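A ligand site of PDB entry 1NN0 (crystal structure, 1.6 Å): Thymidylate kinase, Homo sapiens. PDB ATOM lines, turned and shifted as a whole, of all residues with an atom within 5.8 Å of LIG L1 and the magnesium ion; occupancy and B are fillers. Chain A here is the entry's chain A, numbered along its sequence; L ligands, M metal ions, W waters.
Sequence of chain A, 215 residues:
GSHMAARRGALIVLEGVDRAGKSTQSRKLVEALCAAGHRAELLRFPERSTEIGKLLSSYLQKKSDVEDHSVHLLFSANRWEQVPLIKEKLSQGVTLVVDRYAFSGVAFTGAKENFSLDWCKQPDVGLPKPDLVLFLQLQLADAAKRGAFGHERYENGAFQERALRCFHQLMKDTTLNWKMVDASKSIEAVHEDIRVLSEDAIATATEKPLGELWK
N of Ser 23 sits at hydrogen-bond distance from O5 of LIG L1, at 3.4 Å. O5 of LIG L1 lies within hydrogen-bond range of N of Thr 24 (2.8 Å). An oxygen (O5) of LIG L1 is in hydrogen-bond range of the side-chain hydroxyl of Thr 24, 2.7 Å away. The backbone carbonyl oxygen (O) of Lys 185 sits at hydrogen-bond distance from a nitrogen (N3) of LIG L1, at 2.8 Å. N of Lys 22 is in hydrogen-bond range of O1 of LIG L1 (2.8 Å). An oxygen (O1) of LIG L1 is in salt-bridge range of the side-chain amino group (NZ) of Lys 22 (2.8 Å). The backbone NH (N) of Gly 21 sits at hydrogen-bond distance from an oxygen (O1) of LIG L1, at 3.0 Å. O3 of LIG L1 is in hydrogen-bond range of N of Arg 19, at 3.3 Å. NH2 of Arg 146 lies close to N4 of LIG L1 (3.4 Å). An oxygen (O1) of LIG L1 is in hydrogen-bond range of the backbone NH (N) of Ala 20, 3.4 Å away. O1 of LG2 L2 lies within salt-bridge range of NE of Arg 100, at 2.8 Å.
The side-chain carboxylate (OD2) of Asp 99 lies close to the side-chain hydroxyl (OG) of Ser 23, at 2.5 Å. O of Val 17 is in hydrogen-bond range of NZ of Lys 22 (3.4 Å). NZ of Lys 22 lies within hydrogen-bond range of O of Gly 16 (3.3 Å). The backbone carbonyl oxygen (O) of Arg 19 is in hydrogen-bond range of the guanidinium group (NH1) of Arg 146, 2.8 Å away. NE of Arg 19 is in salt-bridge range of OD2 of Asp 18 (3.7 Å). O of Ala 20 sits at hydrogen-bond distance from NH1 of Arg 146. The backbone carbonyl oxygen of Ala 183 sits at hydrogen-bond distance from the guanidinium group of Arg 146 (2.8 Å). The side-chain amide nitrogen (NE2) of Gln 25 lies within hydrogen-bond range of the backbone carbonyl oxygen (O) of Ile 187, at 3.1 Å.
Residues that only touch LIG L1: Ala 183 (3.8 Å), Ser 186 (3.5 Å) and Ile 187 (3.5 Å). 11 residues have an atom within 4 Å of LIG L1: Arg 19, Ala 20, Gly 21, Lys 22, Ser 23, Thr 24, Arg 146, Ala 183, Lys 185, Ser 186 and Ile 187. The nearest printed residue that does not touch LIG L1 is Val 17 (4.1 Å).
One residue has an atom within 4 Å of the magnesium ion: Ser 23. The nearest printed residue that does not touch the magnesium ion is Asp 99 (4.2 Å).
The magnesium ion is bound by an oxygen (O2) of LIG L1 (2.0 Å), water W5 (2.1 Å), water W11 (2.1 Å), the side-chain hydroxyl (OG) of Ser 23 (2.2 Å), water W8 (2.2 Å) and water W7 (2.2 Å).
Water W8 lies within hydrogen-bond range of OD1 of Asp 99 and O1 of LG2 L2. Water W7 lies within hydrogen-bond range of O3 of LG2 L2 (2.5 Å) and O3 of LIG L1 (2.7 Å). Water W4 lies within hydrogen-bond range of N2 of LIG L1 (2.7 Å), NE2 of Gln 25 (2.9 Å) and O of Ala 20 (3.3 Å). Water W12 lies within hydrogen-bond range of an oxygen (O4) of LIG L1 (2.9 Å), the guanidinium group (NH2) of Arg 27 (3.1 Å) and the side-chain hydroxyl (OG1) of Thr 24 (3.4 Å).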
ATOM      1  N   GLY A  16      12.437 -32.849  -3.929  1.00  0.00           N
ATOM      2  CA  GLY A  16      12.553 -31.931  -2.773  1.00  0.00           C
ATOM      3  C   GLY A  16      11.317 -31.825  -1.913  1.00  0.00           C
ATOM      4  O   GLY A  16      10.295 -32.402  -2.250  1.00  0.00           O
ATOM      5  N   VAL A  17      11.488 -31.111  -0.779  1.00  0.00           N
ATOM      6  CA  VAL A  17      10.317 -31.026   0.119  1.00  0.00           C
ATOM      7  C   VAL A  17       9.191 -30.139  -0.408  1.00  0.00           C
ATOM      8  O   VAL A  17       9.368 -29.315  -1.286  1.00  0.00           O
ATOM      9  CB  VAL A  17      10.775 -30.590   1.519  1.00  0.00           C
ATOM     10  CG1 VAL A  17      11.866 -31.584   1.942  1.00  0.00           C
ATOM     11  CG2 VAL A  17      11.333 -29.193   1.542  1.00  0.00           C
ATOM     12  N   ASP A  18       8.007 -30.331   0.163  1.00  0.00           N
ATOM     13  CA  ASP A  18       6.792 -29.656  -0.307  1.00  0.00           C
ATOM     14  C   ASP A  18       6.911 -28.161  -0.308  1.00  0.00           C
ATOM     15  O   ASP A  18       7.428 -27.560   0.647  1.00  0.00           O
ATOM     16  CB  ASP A  18       5.588 -30.123   0.510  1.00  0.00           C
ATOM     17  CG  ASP A  18       4.274 -29.860  -0.210  1.00  0.00           C
ATOM     18  OD1 ASP A  18       4.138 -30.250  -1.389  1.00  0.00           O
ATOM     19  OD2 ASP A  18       3.397 -29.249   0.440  1.00  0.00           O
ATOM     20  N   ARG A  19       6.572 -27.566  -1.451  1.00  0.00           N
ATOM     21  CA  ARG A  19       6.691 -26.141  -1.636  1.00  0.00           C
ATOM     22  C   ARG A  19       8.122 -25.662  -1.613  1.00  0.00           C
ATOM     23  O   ARG A  19       8.319 -24.457  -1.449  1.00  0.00           O
ATOM     24  CB  ARG A  19       5.905 -25.403  -0.505  1.00  0.00           C
ATOM     25  CG  ARG A  19       4.512 -26.062  -0.544  1.00  0.00           C
ATOM     26  CD  ARG A  19       3.443 -25.103  -0.069  1.00  0.00           C
ATOM     27  NE  ARG A  19       2.714 -25.631   1.071  1.00  0.00           N
ATOM     28  CZ  ARG A  19       3.269 -25.574   2.283  1.00  0.00           C
ATOM     29  NH1 ARG A  19       4.482 -25.047   2.394  1.00  0.00           N
ATOM     30  NH2 ARG A  19       2.654 -26.009   3.368  1.00  0.00           N
ATOM     31  N   ALA A  20       9.073 -26.582  -1.829  1.00  0.00           N
ATOM     32  CA  ALA A  20      10.483 -26.188  -1.850  1.00  0.00           C
ATOM     33  C   ALA A  20      10.832 -25.398  -3.115  1.00  0.00           C
ATOM     34  O   ALA A  20      11.757 -24.602  -3.142  1.00  0.00           O
ATOM     35  CB  ALA A  20      11.357 -27.423  -1.668  1.00  0.00           C
ATOM     36  N   GLY A  21      10.056 -25.591  -4.162  1.00  0.00           N
ATOM     37  CA  GLY A  21      10.145 -24.874  -5.424  1.00  0.00           C
ATOM     38  C   GLY A  21      10.524 -25.755  -6.627  1.00  0.00           C
ATOM     39  O   GLY A  21      11.095 -25.233  -7.595  1.00  0.00           O
ATOM     40  N   LYS A  22      10.195 -27.044  -6.560  1.00  0.00           N
ATOM     41  CA  LYS A  22      10.526 -27.900  -7.716  1.00  0.00           C
ATOM     42  C   LYS A  22       9.971 -27.325  -9.019  1.00  0.00           C
ATOM     43  O   LYS A  22      10.641 -27.489 -10.050  1.00  0.00           O
ATOM     44  CB  LYS A  22      10.095 -29.352  -7.519  1.00  0.00           C
ATOM     45  CG  LYS A  22      10.666 -29.996  -6.264  1.00  0.00           C
ATOM     46  CD  LYS A  22      10.038 -31.317  -5.885  1.00  0.00           C
ATOM     47  CE  LYS A  22       8.532 -31.251  -5.598  1.00  0.00           C
ATOM     48  NZ  LYS A  22       8.354 -30.616  -4.238  1.00  0.00           N
ATOM     49  N   SER A  23       8.661 -27.088  -8.997  1.00  0.00           N
ATOM     50  CA  SER A  23       8.038 -26.631 -10.256  1.00  0.00           C
ATOM     51  C   SER A  23       8.529 -25.284 -10.701  1.00  0.00           C
ATOM     52  O   SER A  23       8.879 -25.082 -11.881  1.00  0.00           O
ATOM     53  CB  SER A  23       6.497 -26.711 -10.180  1.00  0.00           C
ATOM     54  OG  SER A  23       6.217 -28.065  -9.888  1.00  0.00           O
ATOM     55  N   THR A  24       8.695 -24.386  -9.706  1.00  0.00           N
ATOM     56  CA  THR A  24       9.189 -23.055 -10.104  1.00  0.00           C
ATOM     57  C   THR A  24      10.621 -23.164 -10.657  1.00  0.00           C
ATOM     58  O   THR A  24      10.855 -22.581 -11.727  1.00  0.00           O
ATOM     59  CB  THR A  24       9.211 -22.143  -8.862  1.00  0.00           C
ATOM     60  OG1 THR A  24       7.823 -22.020  -8.494  1.00  0.00           O
ATOM     61  CG2 THR A  24       9.718 -20.744  -9.169  1.00  0.00           C
ATOM     62  N   GLN A  25      11.524 -23.846  -9.992  1.00  0.00           N
ATOM     63  CA  GLN A  25      12.924 -23.914 -10.444  1.00  0.00           C
ATOM     64  C   GLN A  25      13.025 -24.780 -11.707  1.00  0.00           C
ATOM     65  O   GLN A  25      13.903 -24.468 -12.513  1.00  0.00           O
ATOM     66  CB  GLN A  25      13.746 -24.473  -9.277  1.00  0.00           C
ATOM     67  CG  GLN A  25      13.743 -23.589  -8.033  1.00  0.00           C
ATOM     68  CD  GLN A  25      14.188 -22.180  -8.395  1.00  0.00           C
ATOM     69  OE1 GLN A  25      14.877 -21.916  -9.373  1.00  0.00           O
ATOM     70  NE2 GLN A  25      13.863 -21.216  -7.508  1.00  0.00           N
ATOM     71  N   ARG A  27      10.789 -24.875 -14.234  1.00  0.00           N
ATOM     72  CA  ARG A  27      10.403 -23.930 -15.295  1.00  0.00           C
ATOM     73  C   ARG A  27      11.495 -22.924 -15.595  1.00  0.00           C
ATOM     74  O   ARG A  27      11.843 -22.713 -16.745  1.00  0.00           O
ATOM     75  CB  ARG A  27       9.123 -23.168 -14.917  1.00  0.00           C
ATOM     76  CG  ARG A  27       7.870 -24.047 -14.953  1.00  0.00           C
ATOM     77  CD  ARG A  27       6.632 -23.164 -14.798  1.00  0.00           C
ATOM     78  NE  ARG A  27       6.626 -22.356 -13.589  1.00  0.00           N
ATOM     79  CZ  ARG A  27       6.059 -22.733 -12.437  1.00  0.00           C
ATOM     80  NH1 ARG A  27       5.453 -23.893 -12.239  1.00  0.00           N
ATOM     81  NH2 ARG A  27       6.066 -21.810 -11.452  1.00  0.00           N
ATOM     82  N   ASP A  99      10.626 -32.530 -13.334  1.00  0.00           N
ATOM     83  CA  ASP A  99      10.043 -32.146 -12.021  1.00  0.00           C
ATOM     84  C   ASP A  99       9.452 -33.428 -11.442  1.00  0.00           C
ATOM     85  O   ASP A  99       8.297 -33.811 -11.838  1.00  0.00           O
ATOM     86  CB  ASP A  99       9.033 -31.073 -12.288  1.00  0.00           C
ATOM     87  CG  ASP A  99       8.210 -30.503 -11.121  1.00  0.00           C
ATOM     88  OD1 ASP A  99       8.374 -30.952  -9.987  1.00  0.00           O
ATOM     89  OD2 ASP A  99       7.354 -29.656 -11.499  1.00  0.00           O
ATOM     90  N   ARG A 100      10.163 -33.966 -10.493  1.00  0.00           N
ATOM     91  CA  ARG A 100       9.936 -35.238  -9.843  1.00  0.00           C
ATOM     92  C   ARG A 100      10.260 -36.428 -10.784  1.00  0.00           C
ATOM     93  O   ARG A 100       9.991 -36.389 -11.973  1.00  0.00           O
ATOM     94  CB  ARG A 100       8.499 -35.483  -9.330  1.00  0.00           C
ATOM     95  CG  ARG A 100       8.211 -34.444  -8.194  1.00  0.00           C
ATOM     96  CD  ARG A 100       6.827 -34.887  -7.658  1.00  0.00           C
ATOM     97  NE  ARG A 100       6.279 -34.009  -6.605  1.00  0.00           N
ATOM     98  CZ  ARG A 100       6.524 -33.996  -5.320  1.00  0.00           C
ATOM     99  NH1 ARG A 100       7.385 -34.804  -4.698  1.00  0.00           N
ATOM    100  NH2 ARG A 100       5.869 -33.046  -4.605  1.00  0.00           N
ATOM    101  N   ARG A 146       5.037 -20.544   2.833  1.00  0.00           N
ATOM    102  CA  ARG A 146       4.794 -20.640   1.397  1.00  0.00           C
ATOM    103  C   ARG A 146       3.319 -20.989   1.204  1.00  0.00           C
ATOM    104  O   ARG A 146       2.918 -21.819   0.402  1.00  0.00           O
ATOM    105  CB  ARG A 146       5.721 -21.565   0.628  1.00  0.00           C
ATOM    106  CG  ARG A 146       7.017 -20.834   0.307  1.00  0.00           C
ATOM    107  CD  ARG A 146       8.113 -21.834  -0.075  1.00  0.00           C
ATOM    108  NE  ARG A 146       9.409 -21.189   0.179  1.00  0.00           N
ATOM    109  CZ  ARG A 146      10.555 -21.640  -0.338  1.00  0.00           C
ATOM    110  NH1 ARG A 146      10.471 -22.708  -1.140  1.00  0.00           N
ATOM    111  NH2 ARG A 146      11.655 -20.987  -0.039  1.00  0.00           N
ATOM    112  N   ALA A 183      16.960 -24.348  -0.688  1.00  0.00           N
ATOM    113  CA  ALA A 183      15.798 -23.715  -1.280  1.00  0.00           C
ATOM    114  C   ALA A 183      15.138 -22.672  -0.384  1.00  0.00           C
ATOM    115  O   ALA A 183      14.058 -22.213  -0.757  1.00  0.00           O
ATOM    116  CB  ALA A 183      14.773 -24.732  -1.793  1.00  0.00           C
ATOM    117  N   SER A 184      15.830 -22.283   0.697  1.00  0.00           N
ATOM    118  CA  SER A 184      15.263 -21.247   1.577  1.00  0.00           C
ATOM    119  C   SER A 184      15.523 -19.856   1.048  1.00  0.00           C
ATOM    120  O   SER A 184      14.954 -18.838   1.486  1.00  0.00           O
ATOM    121  CB  SER A 184      15.831 -21.373   3.015  1.00  0.00           C
ATOM    122  OG  SER A 184      17.166 -20.877   3.034  1.00  0.00           O
ATOM    123  N   LYS A 185      16.465 -19.727   0.109  1.00  0.00           N
ATOM    124  CA  LYS A 185      16.746 -18.427  -0.500  1.00  0.00           C
ATOM    125  C   LYS A 185      15.635 -17.982  -1.420  1.00  0.00           C
ATOM    126  O   LYS A 185      14.622 -18.672  -1.604  1.00  0.00           O
ATOM    127  CB  LYS A 185      18.100 -18.480  -1.230  1.00  0.00           C
ATOM    128  CG  LYS A 185      19.167 -19.009  -0.259  1.00  0.00           C
ATOM    129  CD  LYS A 185      20.580 -18.801  -0.764  1.00  0.00           C
ATOM    130  CE  LYS A 185      20.924 -19.770  -1.889  1.00  0.00           C
ATOM    131  NZ  LYS A 185      22.386 -20.048  -1.905  1.00  0.00           N
ATOM    132  N   SER A 186      15.826 -16.789  -1.997  1.00  0.00           N
ATOM    133  CA  SER A 186      14.871 -16.217  -2.903  1.00  0.00           C
ATOM    134  C   SER A 186      14.749 -17.094  -4.174  1.00  0.00           C
ATOM    135  O   SER A 186      15.708 -17.807  -4.433  1.00  0.00           O
ATOM    136  CB  SER A 186      15.334 -14.831  -3.356  1.00  0.00           C
ATOM    137  OG  SER A 186      16.507 -14.893  -4.171  1.00  0.00           O
ATOM    138  N   ILE A 187      13.690 -16.823  -4.916  1.00  0.00           N
ATOM    139  CA  ILE A 187      13.548 -17.604  -6.170  1.00  0.00           C
ATOM    140  C   ILE A 187      14.771 -17.459  -7.058  1.00  0.00           C
ATOM    141  O   ILE A 187      15.250 -18.459  -7.672  1.00  0.00           O
ATOM    142  CB  ILE A 187      12.271 -17.173  -6.926  1.00  0.00           C
ATOM    143  CG1 ILE A 187      11.058 -17.640  -6.158  1.00  0.00           C
ATOM    144  CG2 ILE A 187      12.341 -17.730  -8.357  1.00  0.00           C
ATOM    145  CD1 ILE A 187       9.700 -17.240  -6.711  1.00  0.00           C
ATOM    146  N   VAL A 190      18.049 -19.211  -5.554  1.00  0.00           N
ATOM    147  CA  VAL A 190      18.002 -20.687  -5.702  1.00  0.00           C
ATOM    148  C   VAL A 190      18.182 -21.029  -7.176  1.00  0.00           C
ATOM    149  O   VAL A 190      18.935 -21.972  -7.474  1.00  0.00           O
ATOM    150  CB  VAL A 190      16.608 -21.168  -5.251  1.00  0.00           C
ATOM    151  CG1 VAL A 190      16.559 -22.674  -5.440  1.00  0.00           C
ATOM    152  CG2 VAL A 190      16.538 -20.861  -3.734  1.00  0.00           C
HETATM  153  P1  LIG L   1       6.857 -27.433  -5.427  1.00  0.00           P
HETATM  154  O1  LIG L   1       8.126 -27.848  -4.855  1.00  0.00           O
HETATM  155  O2  LIG L   1       6.638 -27.737  -6.863  1.00  0.00           O
HETATM  156  O3  LIG L   1       5.551 -27.756  -4.591  1.00  0.00           O
HETATM  157  P2  LIG L   1       6.434 -24.587  -6.230  1.00  0.00           P
HETATM  158  O4  LIG L   1       5.059 -24.891  -6.646  1.00  0.00           O
HETATM  159  O5  LIG L   1       7.575 -24.387  -7.158  1.00  0.00           O
HETATM  160  O6  LIG L   1       6.847 -25.785  -5.285  1.00  0.00           O
HETATM  161  O7  LIG L   1       6.437 -23.420  -5.131  1.00  0.00           O
HETATM  162  C1  LIG L   1       5.482 -23.412  -4.068  1.00  0.00           C
HETATM  163  C2  LIG L   1       5.043 -21.975  -3.809  1.00  0.00           C
HETATM  164  O8  LIG L   1       6.176 -21.284  -3.224  1.00  0.00           O
HETATM  165  C3  LIG L   1       4.633 -21.181  -5.039  1.00  0.00           C
HETATM  166  O9  LIG L   1       3.679 -20.227  -4.638  1.00  0.00           O
HETATM  167  C4  LIG L   1       5.955 -20.475  -5.400  1.00  0.00           C
HETATM  168  O10 LIG L   1       5.808 -19.261  -6.100  1.00  0.00           O
HETATM  169  C5  LIG L   1       6.564 -20.216  -4.011  1.00  0.00           C
HETATM  170  N1  LIG L   1       8.057 -20.253  -4.063  1.00  0.00           N
HETATM  171  C6  LIG L   1       8.796 -21.156  -4.820  1.00  0.00           C
HETATM  172  N2  LIG L   1      10.106 -20.951  -4.593  1.00  0.00           N
HETATM  173  C7  LIG L   1      10.187 -19.946  -3.602  1.00  0.00           C
HETATM  174  C8  LIG L   1      11.270 -19.360  -2.941  1.00  0.00           C
HETATM  175  N3  LIG L   1      12.532 -19.638  -3.127  1.00  0.00           N
HETATM  176  N4  LIG L   1      10.906 -18.406  -2.092  1.00  0.00           N
HETATM  177  C9  LIG L   1       9.634 -18.047  -1.841  1.00  0.00           C
HETATM  178  N5  LIG L   1       8.565 -18.562  -2.425  1.00  0.00           N
HETATM  179  C10 LIG L   1       8.949 -19.512  -3.274  1.00  0.00           C
HETATM  180  P1  LG2 L   2       3.134 -32.273  -7.301  1.00  0.00           P
HETATM  181  O1  LG2 L   2       4.365 -32.606  -8.092  1.00  0.00           O
HETATM  182  O2  LG2 L   2       2.203 -31.328  -7.956  1.00  0.00           O
HETATM  183  O3  LG2 L   2       3.640 -31.925  -5.881  1.00  0.00           O
HETATM  184  O4  LG2 L   2       2.170 -33.483  -7.095  1.00  0.00           O
HETATM  185  N1  LG2 L   2       4.004 -38.742  -6.382  1.00  0.00           N
HETATM  186  C1  LG2 L   2       4.705 -38.326  -7.463  1.00  0.00           C
HETATM  187  C2  LG2 L   2       3.868 -40.073  -5.958  1.00  0.00           C
HETATM  188  O5  LG2 L   2       3.255 -40.453  -4.972  1.00  0.00           O
HETATM  189  N2  LG2 L   2       4.555 -40.965  -6.756  1.00  0.00           N
HETATM  190  C3  LG2 L   2       5.274 -40.638  -7.846  1.00  0.00           C
HETATM  191  O6  LG2 L   2       5.867 -41.519  -8.656  1.00  0.00           O
HETATM  192  C4  LG2 L   2       5.309 -39.262  -8.282  1.00  0.00           C
HETATM  193  C5  LG2 L   2       6.141 -38.960  -9.506  1.00  0.00           C
HETATM  194  C6  LG2 L   2       4.000 -36.826  -4.952  1.00  0.00           C
HETATM  195  C7  LG2 L   2       2.401 -34.825  -7.235  1.00  0.00           C
HETATM  196  C8  LG2 L   2       2.080 -35.741  -6.014  1.00  0.00           C
HETATM  197  O7  LG2 L   2       2.311 -37.072  -6.555  1.00  0.00           O
HETATM  198  C9  LG2 L   2       3.144 -37.781  -5.736  1.00  0.00           C
HETATM  199  C10 LG2 L   2       3.148 -35.583  -4.903  1.00  0.00           C
HETATM  200 MG    MG M   1       5.314 -28.650  -8.017  1.00  0.00          MG
HETATM  201  O   HOH W   1       2.399 -23.845  -6.647  1.00  0.00           O
HETATM  202  O   HOH W   2       1.476 -21.667  -5.144  1.00  0.00           O
HETATM  203  O   HOH W   3      12.514 -17.660   0.036  1.00  0.00           O
HETATM  204  O   HOH W   4      12.573 -22.039  -5.014  1.00  0.00           O
HETATM  205  O   HOH W   5       4.057 -26.943  -8.014  1.00  0.00           O
HETATM  206  O   HOH W   6       6.467 -17.249  -1.566  1.00  0.00           O
HETATM  207  O   HOH W   7       4.333 -29.571  -6.246  1.00  0.00           O
HETATM  208  O   HOH W   8       6.372 -30.546  -8.231  1.00  0.00           O
HETATM  209  O   HOH W   9       6.565 -16.468  -4.610  1.00  0.00           O
HETATM  210  O   HOH W  10       3.124 -26.897  -4.203  1.00  0.00           O
HETATM  211  O   HOH W  11       3.756 -29.472  -9.224  1.00  0.00           O
HETATM  212  O   HOH W  12       4.766 -23.279  -9.092  1.00  0.00           O
